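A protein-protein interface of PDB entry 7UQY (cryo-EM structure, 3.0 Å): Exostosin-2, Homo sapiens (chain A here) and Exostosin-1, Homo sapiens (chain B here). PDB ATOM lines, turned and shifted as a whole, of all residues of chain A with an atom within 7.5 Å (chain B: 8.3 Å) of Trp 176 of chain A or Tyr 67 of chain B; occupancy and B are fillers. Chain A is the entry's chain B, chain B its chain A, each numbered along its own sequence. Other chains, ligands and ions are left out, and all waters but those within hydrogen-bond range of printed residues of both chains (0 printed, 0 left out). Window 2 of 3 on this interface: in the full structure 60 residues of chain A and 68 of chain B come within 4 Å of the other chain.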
ATOM      1  N   LEU A  39     -14.650 -36.126  -3.259  1.00  0.00           N
ATOM      2  CA  LEU A  39     -14.047 -34.803  -3.169  1.00  0.00           C
ATOM      3  C   LEU A  39     -13.126 -34.524  -4.348  1.00  0.00           C
ATOM      4  O   LEU A  39     -12.898 -33.359  -4.694  1.00  0.00           O
ATOM      5  CB  LEU A  39     -13.288 -34.663  -1.852  1.00  0.00           C
ATOM      6  CG  LEU A  39     -12.897 -33.241  -1.456  1.00  0.00           C
ATOM      7  CD1 LEU A  39     -14.132 -32.417  -1.135  1.00  0.00           C
ATOM      8  CD2 LEU A  39     -11.946 -33.271  -0.281  1.00  0.00           C
ATOM      9  N   ASP A 154     -21.702 -34.605  14.980  1.00  0.00           N
ATOM     10  CA  ASP A 154     -20.483 -34.072  14.396  1.00  0.00           C
ATOM     11  C   ASP A 154     -20.842 -33.141  13.248  1.00  0.00           C
ATOM     12  O   ASP A 154     -21.816 -33.368  12.526  1.00  0.00           O
ATOM     13  CB  ASP A 154     -19.554 -35.190  13.902  1.00  0.00           C
ATOM     14  CG  ASP A 154     -18.241 -34.661  13.361  1.00  0.00           C
ATOM     15  OD1 ASP A 154     -17.444 -34.119  14.156  1.00  0.00           O
ATOM     16  OD2 ASP A 154     -18.003 -34.786  12.142  1.00  0.00           O
ATOM     17  N   TYR A 155     -20.043 -32.092  13.087  1.00  0.00           N
ATOM     18  CA  TYR A 155     -20.258 -31.083  12.051  1.00  0.00           C
ATOM     19  C   TYR A 155     -19.353 -31.427  10.873  1.00  0.00           C
ATOM     20  O   TYR A 155     -18.175 -31.062  10.854  1.00  0.00           O
ATOM     21  CB  TYR A 155     -19.977 -29.685  12.592  1.00  0.00           C
ATOM     22  CG  TYR A 155     -20.951 -29.214  13.654  1.00  0.00           C
ATOM     23  CD1 TYR A 155     -22.017 -30.008  14.055  1.00  0.00           C
ATOM     24  CD2 TYR A 155     -20.787 -27.981  14.271  1.00  0.00           C
ATOM     25  CE1 TYR A 155     -22.901 -29.583  15.028  1.00  0.00           C
ATOM     26  CE2 TYR A 155     -21.664 -27.549  15.247  1.00  0.00           C
ATOM     27  CZ  TYR A 155     -22.720 -28.352  15.621  1.00  0.00           C
ATOM     28  OH  TYR A 155     -23.597 -27.925  16.592  1.00  0.00           O
ATOM     29  N   ASN A 156     -19.908 -32.131   9.887  1.00  0.00           N
ATOM     30  CA  ASN A 156     -19.137 -32.555   8.728  1.00  0.00           C
ATOM     31  C   ASN A 156     -18.864 -31.424   7.747  1.00  0.00           C
ATOM     32  O   ASN A 156     -18.078 -31.617   6.813  1.00  0.00           O
ATOM     33  CB  ASN A 156     -19.857 -33.695   8.003  1.00  0.00           C
ATOM     34  CG  ASN A 156     -19.719 -35.022   8.722  1.00  0.00           C
ATOM     35  OD1 ASN A 156     -18.737 -35.262   9.422  1.00  0.00           O
ATOM     36  ND2 ASN A 156     -20.708 -35.893   8.551  1.00  0.00           N
ATOM     37  N   THR A 157     -19.501 -30.267   7.930  1.00  0.00           N
ATOM     38  CA  THR A 157     -19.294 -29.078   7.104  1.00  0.00           C
ATOM     39  C   THR A 157     -19.650 -29.334   5.639  1.00  0.00           C
ATOM     40  O   THR A 157     -19.203 -28.614   4.739  1.00  0.00           O
ATOM     41  CB  THR A 157     -17.854 -28.565   7.242  1.00  0.00           C
ATOM     42  OG1 THR A 157     -17.467 -28.624   8.620  1.00  0.00           O
ATOM     43  CG2 THR A 157     -17.765 -27.116   6.817  1.00  0.00           C
ATOM     44  N   ALA A 158     -20.454 -30.361   5.382  1.00  0.00           N
ATOM     45  CA  ALA A 158     -20.925 -30.663   4.040  1.00  0.00           C
ATOM     46  C   ALA A 158     -22.153 -31.549   4.160  1.00  0.00           C
ATOM     47  O   ALA A 158     -22.439 -32.101   5.226  1.00  0.00           O
ATOM     48  CB  ALA A 158     -19.842 -31.344   3.196  1.00  0.00           C
ATOM     49  N   PHE A 173     -19.278 -24.148   4.200  1.00  0.00           N
ATOM     50  CA  PHE A 173     -18.159 -24.756   3.494  1.00  0.00           C
ATOM     51  C   PHE A 173     -16.851 -24.465   4.209  1.00  0.00           C
ATOM     52  O   PHE A 173     -16.528 -23.305   4.480  1.00  0.00           O
ATOM     53  CB  PHE A 173     -18.065 -24.264   2.050  1.00  0.00           C
ATOM     54  CG  PHE A 173     -18.893 -25.048   1.085  1.00  0.00           C
ATOM     55  CD1 PHE A 173     -18.901 -26.430   1.134  1.00  0.00           C
ATOM     56  CD2 PHE A 173     -19.638 -24.412   0.111  1.00  0.00           C
ATOM     57  CE1 PHE A 173     -19.646 -27.160   0.242  1.00  0.00           C
ATOM     58  CE2 PHE A 173     -20.388 -25.139  -0.782  1.00  0.00           C
ATOM     59  CZ  PHE A 173     -20.388 -26.513  -0.717  1.00  0.00           C
ATOM     60  N   SER A 174     -16.102 -25.521   4.497  1.00  0.00           N
ATOM     61  CA  SER A 174     -14.703 -25.421   4.872  1.00  0.00           C
ATOM     62  C   SER A 174     -13.843 -25.662   3.641  1.00  0.00           C
ATOM     63  O   SER A 174     -14.299 -26.206   2.634  1.00  0.00           O
ATOM     64  CB  SER A 174     -14.351 -26.430   5.967  1.00  0.00           C
ATOM     65  OG  SER A 174     -14.649 -27.751   5.551  1.00  0.00           O
ATOM     66  N   THR A 175     -12.581 -25.248   3.732  1.00  0.00           N
ATOM     67  CA  THR A 175     -11.679 -25.408   2.602  1.00  0.00           C
ATOM     68  C   THR A 175     -11.395 -26.872   2.289  1.00  0.00           C
ATOM     69  O   THR A 175     -10.902 -27.174   1.199  1.00  0.00           O
ATOM     70  CB  THR A 175     -10.373 -24.667   2.869  1.00  0.00           C
ATOM     71  OG1 THR A 175      -9.625 -24.555   1.651  1.00  0.00           O
ATOM     72  CG2 THR A 175      -9.560 -25.413   3.896  1.00  0.00           C
ATOM     73  N   TRP A 176     -11.696 -27.783   3.215  1.00  0.00           N
ATOM     74  CA  TRP A 176     -11.526 -29.208   2.969  1.00  0.00           C
ATOM     75  C   TRP A 176     -12.779 -29.855   2.405  1.00  0.00           C
ATOM     76  O   TRP A 176     -12.690 -30.910   1.767  1.00  0.00           O
ATOM     77  CB  TRP A 176     -11.124 -29.925   4.260  1.00  0.00           C
ATOM     78  CG  TRP A 176      -9.819 -29.466   4.812  1.00  0.00           C
ATOM     79  CD1 TRP A 176      -8.578 -29.805   4.365  1.00  0.00           C
ATOM     80  CD2 TRP A 176      -9.621 -28.575   5.913  1.00  0.00           C
ATOM     81  NE1 TRP A 176      -7.617 -29.182   5.122  1.00  0.00           N
ATOM     82  CE2 TRP A 176      -8.232 -28.421   6.080  1.00  0.00           C
ATOM     83  CE3 TRP A 176     -10.484 -27.894   6.775  1.00  0.00           C
ATOM     84  CZ2 TRP A 176      -7.687 -27.613   7.073  1.00  0.00           C
ATOM     85  CZ3 TRP A 176      -9.940 -27.094   7.759  1.00  0.00           C
ATOM     86  CH2 TRP A 176      -8.556 -26.960   7.900  1.00  0.00           C
ATOM     87  N   THR A 177     -13.944 -29.254   2.632  1.00  0.00           N
ATOM     88  CA  THR A 177     -15.209 -29.790   2.155  1.00  0.00           C
ATOM     89  C   THR A 177     -15.714 -29.079   0.908  1.00  0.00           C
ATOM     90  O   THR A 177     -16.812 -29.389   0.433  1.00  0.00           O
ATOM     91  CB  THR A 177     -16.265 -29.709   3.258  1.00  0.00           C
ATOM     92  OG1 THR A 177     -16.384 -28.352   3.704  1.00  0.00           O
ATOM     93  CG2 THR A 177     -15.876 -30.592   4.431  1.00  0.00           C
ATOM     94  N   TYR A 178     -14.947 -28.138   0.369  1.00  0.00           N
ATOM     95  CA  TYR A 178     -15.370 -27.340  -0.774  1.00  0.00           C
ATOM     96  C   TYR A 178     -14.523 -27.684  -1.989  1.00  0.00           C
ATOM     97  O   TYR A 178     -13.301 -27.497  -1.974  1.00  0.00           O
ATOM     98  CB  TYR A 178     -15.272 -25.848  -0.461  1.00  0.00           C
ATOM     99  CG  TYR A 178     -15.539 -24.956  -1.648  1.00  0.00           C
ATOM    100  CD1 TYR A 178     -16.833 -24.733  -2.097  1.00  0.00           C
ATOM    101  CD2 TYR A 178     -14.500 -24.309  -2.301  1.00  0.00           C
ATOM    102  CE1 TYR A 178     -17.083 -23.907  -3.175  1.00  0.00           C
ATOM    103  CE2 TYR A 178     -14.741 -23.480  -3.376  1.00  0.00           C
ATOM    104  CZ  TYR A 178     -16.033 -23.284  -3.810  1.00  0.00           C
ATOM    105  OH  TYR A 178     -16.275 -22.460  -4.885  1.00  0.00           O
ATOM    106  N   ARG A 179     -15.174 -28.185  -3.033  1.00  0.00           N
ATOM    107  CA  ARG A 179     -14.527 -28.362  -4.322  1.00  0.00           C
ATOM    108  C   ARG A 179     -14.500 -27.023  -5.047  1.00  0.00           C
ATOM    109  O   ARG A 179     -15.541 -26.385  -5.226  1.00  0.00           O
ATOM    110  CB  ARG A 179     -15.268 -29.420  -5.136  1.00  0.00           C
ATOM    111  CG  ARG A 179     -15.306 -30.775  -4.448  1.00  0.00           C
ATOM    112  CD  ARG A 179     -16.334 -31.700  -5.065  1.00  0.00           C
ATOM    113  NE  ARG A 179     -17.650 -31.517  -4.468  1.00  0.00           N
ATOM    114  CZ  ARG A 179     -18.735 -32.191  -4.824  1.00  0.00           C
ATOM    115  NH1 ARG A 179     -18.695 -33.113  -5.770  1.00  0.00           N
ATOM    116  NH2 ARG A 179     -19.887 -31.935  -4.212  1.00  0.00           N
ATOM    117  N   ASP A 302     -12.926 -20.242  11.588  1.00  0.00           N
ATOM    118  CA  ASP A 302     -11.525 -20.550  11.321  1.00  0.00           C
ATOM    119  C   ASP A 302     -11.293 -20.851   9.846  1.00  0.00           C
ATOM    120  O   ASP A 302     -10.543 -20.142   9.165  1.00  0.00           O
ATOM    121  CB  ASP A 302     -11.076 -21.725  12.191  1.00  0.00           C
ATOM    122  CG  ASP A 302      -9.579 -21.735  12.424  1.00  0.00           C
ATOM    123  OD1 ASP A 302      -8.994 -20.643  12.584  1.00  0.00           O
ATOM    124  OD2 ASP A 302      -8.987 -22.835  12.452  1.00  0.00           O
ATOM    125  N   SER A 303     -11.927 -21.901   9.333  1.00  0.00           N
ATOM    126  CA  SER A 303     -11.766 -22.318   7.941  1.00  0.00           C
ATOM    127  C   SER A 303     -13.134 -22.265   7.278  1.00  0.00           C
ATOM    128  O   SER A 303     -13.819 -23.282   7.155  1.00  0.00           O
ATOM    129  CB  SER A 303     -11.159 -23.708   7.861  1.00  0.00           C
ATOM    130  OG  SER A 303     -12.050 -24.679   8.380  1.00  0.00           O
ATOM    131  N   TYR A 304     -13.521 -21.072   6.833  1.00  0.00           N
ATOM    132  CA  TYR A 304     -14.823 -20.841   6.226  1.00  0.00           C
ATOM    133  C   TYR A 304     -14.655 -19.935   5.019  1.00  0.00           C
ATOM    134  O   TYR A 304     -13.969 -18.911   5.098  1.00  0.00           O
ATOM    135  CB  TYR A 304     -15.792 -20.210   7.231  1.00  0.00           C
ATOM    136  CG  TYR A 304     -17.141 -19.840   6.657  1.00  0.00           C
ATOM    137  CD1 TYR A 304     -17.884 -20.758   5.927  1.00  0.00           C
ATOM    138  CD2 TYR A 304     -17.670 -18.572   6.848  1.00  0.00           C
ATOM    139  CE1 TYR A 304     -19.117 -20.421   5.405  1.00  0.00           C
ATOM    140  CE2 TYR A 304     -18.899 -18.226   6.329  1.00  0.00           C
ATOM    141  CZ  TYR A 304     -19.618 -19.154   5.609  1.00  0.00           C
ATOM    142  OH  TYR A 304     -20.845 -18.812   5.090  1.00  0.00           O
ATOM    143  N   ILE A 305     -15.285 -20.306   3.909  1.00  0.00           N
ATOM    144  CA  ILE A 305     -15.293 -19.489   2.703  1.00  0.00           C
ATOM    145  C   ILE A 305     -16.638 -18.778   2.631  1.00  0.00           C
ATOM    146  O   ILE A 305     -17.696 -19.409   2.745  1.00  0.00           O
ATOM    147  CB  ILE A 305     -15.020 -20.324   1.443  1.00  0.00           C
ATOM    148  CG1 ILE A 305     -16.103 -21.377   1.231  1.00  0.00           C
ATOM    149  CG2 ILE A 305     -13.657 -20.994   1.537  1.00  0.00           C
ATOM    150  CD1 ILE A 305     -16.011 -22.050  -0.091  1.00  0.00           C
ATOM    151  N   SER B  64      -6.449 -30.286  12.725  1.00  0.00           N
ATOM    152  CA  SER B  64      -5.174 -29.905  12.129  1.00  0.00           C
ATOM    153  C   SER B  64      -4.325 -31.134  11.823  1.00  0.00           C
ATOM    154  O   SER B  64      -3.802 -31.280  10.719  1.00  0.00           O
ATOM    155  CB  SER B  64      -4.412 -28.956  13.056  1.00  0.00           C
ATOM    156  OG  SER B  64      -3.182 -28.555  12.477  1.00  0.00           O
ATOM    157  N   SER B  65      -4.189 -32.017  12.816  1.00  0.00           N
ATOM    158  CA  SER B  65      -3.399 -33.229  12.625  1.00  0.00           C
ATOM    159  C   SER B  65      -4.061 -34.188  11.645  1.00  0.00           C
ATOM    160  O   SER B  65      -3.367 -34.956  10.969  1.00  0.00           O
ATOM    161  CB  SER B  65      -3.167 -33.920  13.969  1.00  0.00           C
ATOM    162  OG  SER B  65      -2.435 -35.122  13.805  1.00  0.00           O
ATOM    163  N   ILE B  66      -5.393 -34.165  11.559  1.00  0.00           N
ATOM    164  CA  ILE B  66      -6.100 -35.075  10.661  1.00  0.00           C
ATOM    165  C   ILE B  66      -5.767 -34.766   9.207  1.00  0.00           C
ATOM    166  O   ILE B  66      -5.551 -35.678   8.399  1.00  0.00           O
ATOM    167  CB  ILE B  66      -7.615 -35.005  10.924  1.00  0.00           C
ATOM    168  CG1 ILE B  66      -7.941 -35.545  12.318  1.00  0.00           C
ATOM    169  CG2 ILE B  66      -8.381 -35.778   9.861  1.00  0.00           C
ATOM    170  CD1 ILE B  66      -9.410 -35.470  12.675  1.00  0.00           C
ATOM    171  N   TYR B  67      -5.706 -33.483   8.851  1.00  0.00           N
ATOM    172  CA  TYR B  67      -5.505 -33.053   7.474  1.00  0.00           C
ATOM    173  C   TYR B  67      -4.050 -32.705   7.177  1.00  0.00           C
ATOM    174  O   TYR B  67      -3.778 -31.790   6.392  1.00  0.00           O
ATOM    175  CB  TYR B  67      -6.409 -31.862   7.158  1.00  0.00           C
ATOM    176  CG  TYR B  67      -7.820 -32.012   7.680  1.00  0.00           C
ATOM    177  CD1 TYR B  67      -8.656 -33.007   7.197  1.00  0.00           C
ATOM    178  CD2 TYR B  67      -8.314 -31.155   8.654  1.00  0.00           C
ATOM    179  CE1 TYR B  67      -9.947 -33.146   7.669  1.00  0.00           C
ATOM    180  CE2 TYR B  67      -9.603 -31.287   9.134  1.00  0.00           C
ATOM    181  CZ  TYR B  67     -10.415 -32.284   8.638  1.00  0.00           C
ATOM    182  OH  TYR B  67     -11.699 -32.420   9.111  1.00  0.00           O
ATOM    183  N   LYS B  68      -3.106 -33.417   7.790  1.00  0.00           N
ATOM    184  CA  LYS B  68      -1.683 -33.181   7.554  1.00  0.00           C
ATOM    185  C   LYS B  68      -1.166 -34.159   6.498  1.00  0.00           C
ATOM    186  O   LYS B  68      -0.392 -35.077   6.767  1.00  0.00           O
ATOM    187  CB  LYS B  68      -0.904 -33.296   8.862  1.00  0.00           C
ATOM    188  CG  LYS B  68      -0.732 -31.973   9.592  1.00  0.00           C
ATOM    189  CD  LYS B  68      -0.239 -32.178  11.014  1.00  0.00           C
ATOM    190  CE  LYS B  68      -0.208 -30.862  11.776  1.00  0.00           C
ATOM    191  NZ  LYS B  68       0.273 -31.035  13.174  1.00  0.00           N
ATOM    192  N   GLY B  69      -1.624 -33.937   5.272  1.00  0.00           N
ATOM    193  CA  GLY B  69      -1.242 -34.768   4.135  1.00  0.00           C
ATOM    194  C   GLY B  69      -1.355 -33.989   2.854  1.00  0.00           C
ATOM    195  O   GLY B  69      -0.905 -32.838   2.773  1.00  0.00           O
ATOM    196  N   LYS B  70      -1.945 -34.614   1.834  1.00  0.00           N
ATOM    197  CA  LYS B  70      -2.254 -33.883   0.610  1.00  0.00           C
ATOM    198  C   LYS B  70      -3.337 -32.832   0.832  1.00  0.00           C
ATOM    199  O   LYS B  70      -3.541 -31.975  -0.033  1.00  0.00           O
ATOM    200  CB  LYS B  70      -2.652 -34.863  -0.501  1.00  0.00           C
ATOM    201  CG  LYS B  70      -3.928 -35.667  -0.259  1.00  0.00           C
ATOM    202  CD  LYS B  70      -5.177 -34.976  -0.791  1.00  0.00           C
ATOM    203  CE  LYS B  70      -6.404 -35.858  -0.623  1.00  0.00           C
ATOM    204  NZ  LYS B  70      -7.642 -35.198  -1.117  1.00  0.00           N
ATOM    205  N   LYS B  71      -4.037 -32.886   1.966  1.00  0.00           N
ATOM    206  CA  LYS B  71      -5.098 -31.947   2.294  1.00  0.00           C
ATOM    207  C   LYS B  71      -4.617 -30.759   3.123  1.00  0.00           C
ATOM    208  O   LYS B  71      -5.441 -30.101   3.765  1.00  0.00           O
ATOM    209  CB  LYS B  71      -6.222 -32.669   3.040  1.00  0.00           C
ATOM    210  CG  LYS B  71      -7.001 -33.656   2.201  1.00  0.00           C
ATOM    211  CD  LYS B  71      -8.041 -34.375   3.039  1.00  0.00           C
ATOM    212  CE  LYS B  71      -9.170 -33.438   3.432  1.00  0.00           C
ATOM    213  NZ  LYS B  71      -9.985 -33.018   2.265  1.00  0.00           N
ATOM    214  N   CYS B  72      -3.318 -30.466   3.129  1.00  0.00           N
ATOM    215  CA  CYS B  72      -2.831 -29.333   3.904  1.00  0.00           C
ATOM    216  C   CYS B  72      -3.306 -28.008   3.334  1.00  0.00           C
ATOM    217  O   CYS B  72      -3.296 -27.792   2.119  1.00  0.00           O
ATOM    218  CB  CYS B  72      -1.308 -29.337   3.995  1.00  0.00           C
ATOM    219  SG  CYS B  72      -0.609 -30.690   4.925  1.00  0.00           S
ATOM    220  N   ARG B  73      -3.728 -27.126   4.232  1.00  0.00           N
ATOM    221  CA  ARG B  73      -4.007 -25.731   3.952  1.00  0.00           C
ATOM    222  C   ARG B  73      -3.237 -24.908   4.977  1.00  0.00           C
ATOM    223  O   ARG B  73      -2.613 -25.454   5.892  1.00  0.00           O
ATOM    224  CB  ARG B  73      -5.511 -25.450   4.008  1.00  0.00           C
ATOM    225  CG  ARG B  73      -6.339 -26.489   3.282  1.00  0.00           C
ATOM    226  CD  ARG B  73      -6.341 -26.294   1.784  1.00  0.00           C
ATOM    227  NE  ARG B  73      -7.401 -27.071   1.153  1.00  0.00           N
ATOM    228  CZ  ARG B  73      -7.260 -28.313   0.711  1.00  0.00           C
ATOM    229  NH1 ARG B  73      -6.114 -28.960   0.826  1.00  0.00           N
ATOM    230  NH2 ARG B  73      -8.297 -28.922   0.144  1.00  0.00           N
ATOM    231  N   MET B  74      -3.277 -23.583   4.841  1.00  0.00           N
ATOM    232  CA  MET B  74      -2.409 -22.767   5.678  1.00  0.00           C
ATOM    233  C   MET B  74      -2.871 -22.702   7.128  1.00  0.00           C
ATOM    234  O   MET B  74      -2.071 -22.368   8.007  1.00  0.00           O
ATOM    235  CB  MET B  74      -2.271 -21.366   5.090  1.00  0.00           C
ATOM    236  CG  MET B  74      -1.530 -21.367   3.773  1.00  0.00           C
ATOM    237  SD  MET B  74      -1.408 -19.756   3.005  1.00  0.00           S
ATOM    238  CE  MET B  74      -0.253 -18.945   4.105  1.00  0.00           C
ATOM    239  N   GLU B  75      -4.132 -23.012   7.415  1.00  0.00           N
ATOM    240  CA  GLU B  75      -4.544 -23.066   8.810  1.00  0.00           C
ATOM    241  C   GLU B  75      -4.156 -24.371   9.496  1.00  0.00           C
ATOM    242  O   GLU B  75      -4.258 -24.456  10.725  1.00  0.00           O
ATOM    243  CB  GLU B  75      -6.053 -22.843   8.932  1.00  0.00           C
ATOM    244  CG  GLU B  75      -6.900 -23.866   8.214  1.00  0.00           C
ATOM    245  CD  GLU B  75      -7.322 -23.396   6.841  1.00  0.00           C
ATOM    246  OE1 GLU B  75      -6.673 -22.479   6.296  1.00  0.00           O
ATOM    247  OE2 GLU B  75      -8.313 -23.937   6.312  1.00  0.00           O
ATOM    248  N   SER B  76      -3.718 -25.385   8.747  1.00  0.00           N
ATOM    249  CA  SER B  76      -3.274 -26.640   9.346  1.00  0.00           C
ATOM    250  C   SER B  76      -1.788 -26.889   9.119  1.00  0.00           C
ATOM    251  O   SER B  76      -1.042 -27.042  10.092  1.00  0.00           O
ATOM    252  CB  SER B  76      -4.104 -27.807   8.797  1.00  0.00           C
ATOM    253  OG  SER B  76      -3.830 -28.025   7.425  1.00  0.00           O
ATOM    254  N   CYS B  77      -1.331 -26.934   7.872  1.00  0.00           N
ATOM    255  CA  CYS B  77       0.081 -27.173   7.570  1.00  0.00           C
ATOM    256  C   CYS B  77       0.811 -25.861   7.280  1.00  0.00           C
ATOM    257  O   CYS B  77       1.402 -25.666   6.219  1.00  0.00           O
ATOM    258  CB  CYS B  77       0.215 -28.162   6.412  1.00  0.00           C
ATOM    259  SG  CYS B  77      -0.382 -29.847   6.768  1.00  0.00           S
ATOM    260  N   GLY B 186       5.798 -33.534   2.164  1.00  0.00           N
ATOM    261  CA  GLY B 186       5.235 -33.440   3.495  1.00  0.00           C
ATOM    262  C   GLY B 186       4.296 -32.264   3.659  1.00  0.00           C
ATOM    263  O   GLY B 186       3.233 -32.215   3.033  1.00  0.00           O
ATOM    264  N   GLN B 187       4.678 -31.308   4.501  1.00  0.00           N
ATOM    265  CA  GLN B 187       3.872 -30.124   4.757  1.00  0.00           C
ATOM    266  C   GLN B 187       4.234 -28.951   3.858  1.00  0.00           C
ATOM    267  O   GLN B 187       3.662 -27.868   4.019  1.00  0.00           O
ATOM    268  CB  GLN B 187       4.010 -29.699   6.222  1.00  0.00           C
ATOM    269  CG  GLN B 187       3.153 -30.495   7.189  1.00  0.00           C
ATOM    270  CD  GLN B 187       3.147 -29.901   8.584  1.00  0.00           C
ATOM    271  OE1 GLN B 187       4.008 -29.092   8.930  1.00  0.00           O
ATOM    272  NE2 GLN B 187       2.173 -30.300   9.392  1.00  0.00           N
ATOM    273  N   ARG B 201      -4.183 -27.673  -4.245  1.00  0.00           N
ATOM    274  CA  ARG B 201      -4.670 -27.147  -2.980  1.00  0.00           C
ATOM    275  C   ARG B 201      -5.274 -25.768  -3.213  1.00  0.00           C
ATOM    276  O   ARG B 201      -4.584 -24.883  -3.729  1.00  0.00           O
ATOM    277  CB  ARG B 201      -3.539 -27.073  -1.969  1.00  0.00           C
ATOM    278  CG  ARG B 201      -3.424 -28.300  -1.079  1.00  0.00           C
ATOM    279  CD  ARG B 201      -2.632 -29.412  -1.749  1.00  0.00           C
ATOM    280  NE  ARG B 201      -1.211 -29.099  -1.836  1.00  0.00           N
ATOM    281  CZ  ARG B 201      -0.338 -29.300  -0.858  1.00  0.00           C
ATOM    282  NH1 ARG B 201      -0.707 -29.815   0.303  1.00  0.00           N
ATOM    283  NH2 ARG B 201       0.937 -28.978  -1.051  1.00  0.00           N
ATOM    284  N   PRO B 202      -6.542 -25.544  -2.858  1.00  0.00           N
ATOM    285  CA  PRO B 202      -7.212 -24.296  -3.260  1.00  0.00           C
ATOM    286  C   PRO B 202      -6.521 -23.033  -2.782  1.00  0.00           C
ATOM    287  O   PRO B 202      -6.526 -22.029  -3.505  1.00  0.00           O
ATOM    288  CB  PRO B 202      -8.610 -24.441  -2.643  1.00  0.00           C
ATOM    289  CG  PRO B 202      -8.812 -25.914  -2.521  1.00  0.00           C
ATOM    290  CD  PRO B 202      -7.463 -26.474  -2.185  1.00  0.00           C
ATOM    291  N   PHE B 204      -3.280 -23.232  -0.849  1.00  0.00           N
ATOM    292  CA  PHE B 204      -1.962 -23.596  -0.345  1.00  0.00           C
ATOM    293  C   PHE B 204      -0.906 -23.596  -1.438  1.00  0.00           C
ATOM    294  O   PHE B 204       0.178 -23.033  -1.245  1.00  0.00           O
ATOM    295  CB  PHE B 204      -2.019 -24.973   0.337  1.00  0.00           C
ATOM    296  CG  PHE B 204      -0.885 -25.229   1.285  1.00  0.00           C
ATOM    297  CD1 PHE B 204      -0.393 -24.217   2.089  1.00  0.00           C
ATOM    298  CD2 PHE B 204      -0.313 -26.485   1.376  1.00  0.00           C
ATOM    299  CE1 PHE B 204       0.648 -24.451   2.962  1.00  0.00           C
ATOM    300  CE2 PHE B 204       0.727 -26.726   2.247  1.00  0.00           C
ATOM    301  CZ  PHE B 204       1.209 -25.708   3.040  1.00  0.00           C
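Printed residues of chain B within 4 Å of Leu 39 of chain A: Lys 71.
Thr 175 of chain A touches just these residues of chain B: Arg 73 and Glu 75.
Printed residues of chain B within 4 Å of Ser 303 of chain A: Glu 75 (3.2 Å).
Ser 65 of chain B touches none of the printed residues of chain A.
Tyr 67 of chain B touches just one residue of chain A: Trp 176 (3.6 Å).
Printed residues of chain A within 4 Å of Lys 71 of chain B: Leu 39 and Trp 176.
Printed residues of chain A within 4 Å of Arg 73 of chain B: Thr 175 (3.3 Å) and Trp 176 (3.5 Å).
Of the printed residues of chain A, Ser 76 of chain B touches Trp 176 (3.9 Å).
Cys 77 of chain B touches none of the printed residues of chain A.
The nearest printed residue of chain B that does not touch Ser 303 of chain A is Arg 73 of chain B (7.1 Å).
The guanidinium group (NH1) of Arg 73 of chain B lies within hydrogen-bond range of the backbone carbonyl oxygen (O) of Lys 71 of chain B (3.2 Å).
The backbone carbonyl oxygen of Arg 73 of chain B is in hydrogen-bond range of the side-chain hydroxyl of Ser 76 of chain B (3.2 Å).
The side-chain sulfur of Cys 72 of chain B forms a disulfide with the side-chain sulfur of Cys 77 of chain B (2.0 Å).
NZ of Lys 71 of chain B touches CD2 of Leu 39 of chain A, 3.2 Å away.
Thr 175 of chain A touches Glu 75 of chain B (CG2 to OE2, 3.1 Å).
Trp 176 of chain A touches Tyr 67 of chain B (NE1 to CB, 3.6 Å).
Trp 176 of chain A touches Arg 73 of chain B (NE1 to CG, 3.5 Å).
CH2 of Trp 176 of chain A touches OE2 of Glu 75 of chain B, 3.4 Å away.
CZ2 of Trp 176 of chain A touches OG of Ser 76 of chain B, at 3.9 Å.
Glu 75 of chain B touches Ser 303 of chain A (OE2 to CB, 3.2 Å).
Hydrophobic or aromatic side chains of chain A that line the printed part of chain B: Leu 39 and Trp 176.
Hydrophobic or aromatic side chains of chain B within 4 Å of the printed part of chain A: Tyr 67.
Among the printed residues, 9 pairs touch across the chains.
O of Lys 71 of chain B is in hydrogen-bond range of NE1 of Trp 176 of chain A, at 2.7 Å.
The backbone carbonyl oxygen of Thr 175 of chain A lies within hydrogen-bond range of the guanidinium group of Arg 73 of chain B.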
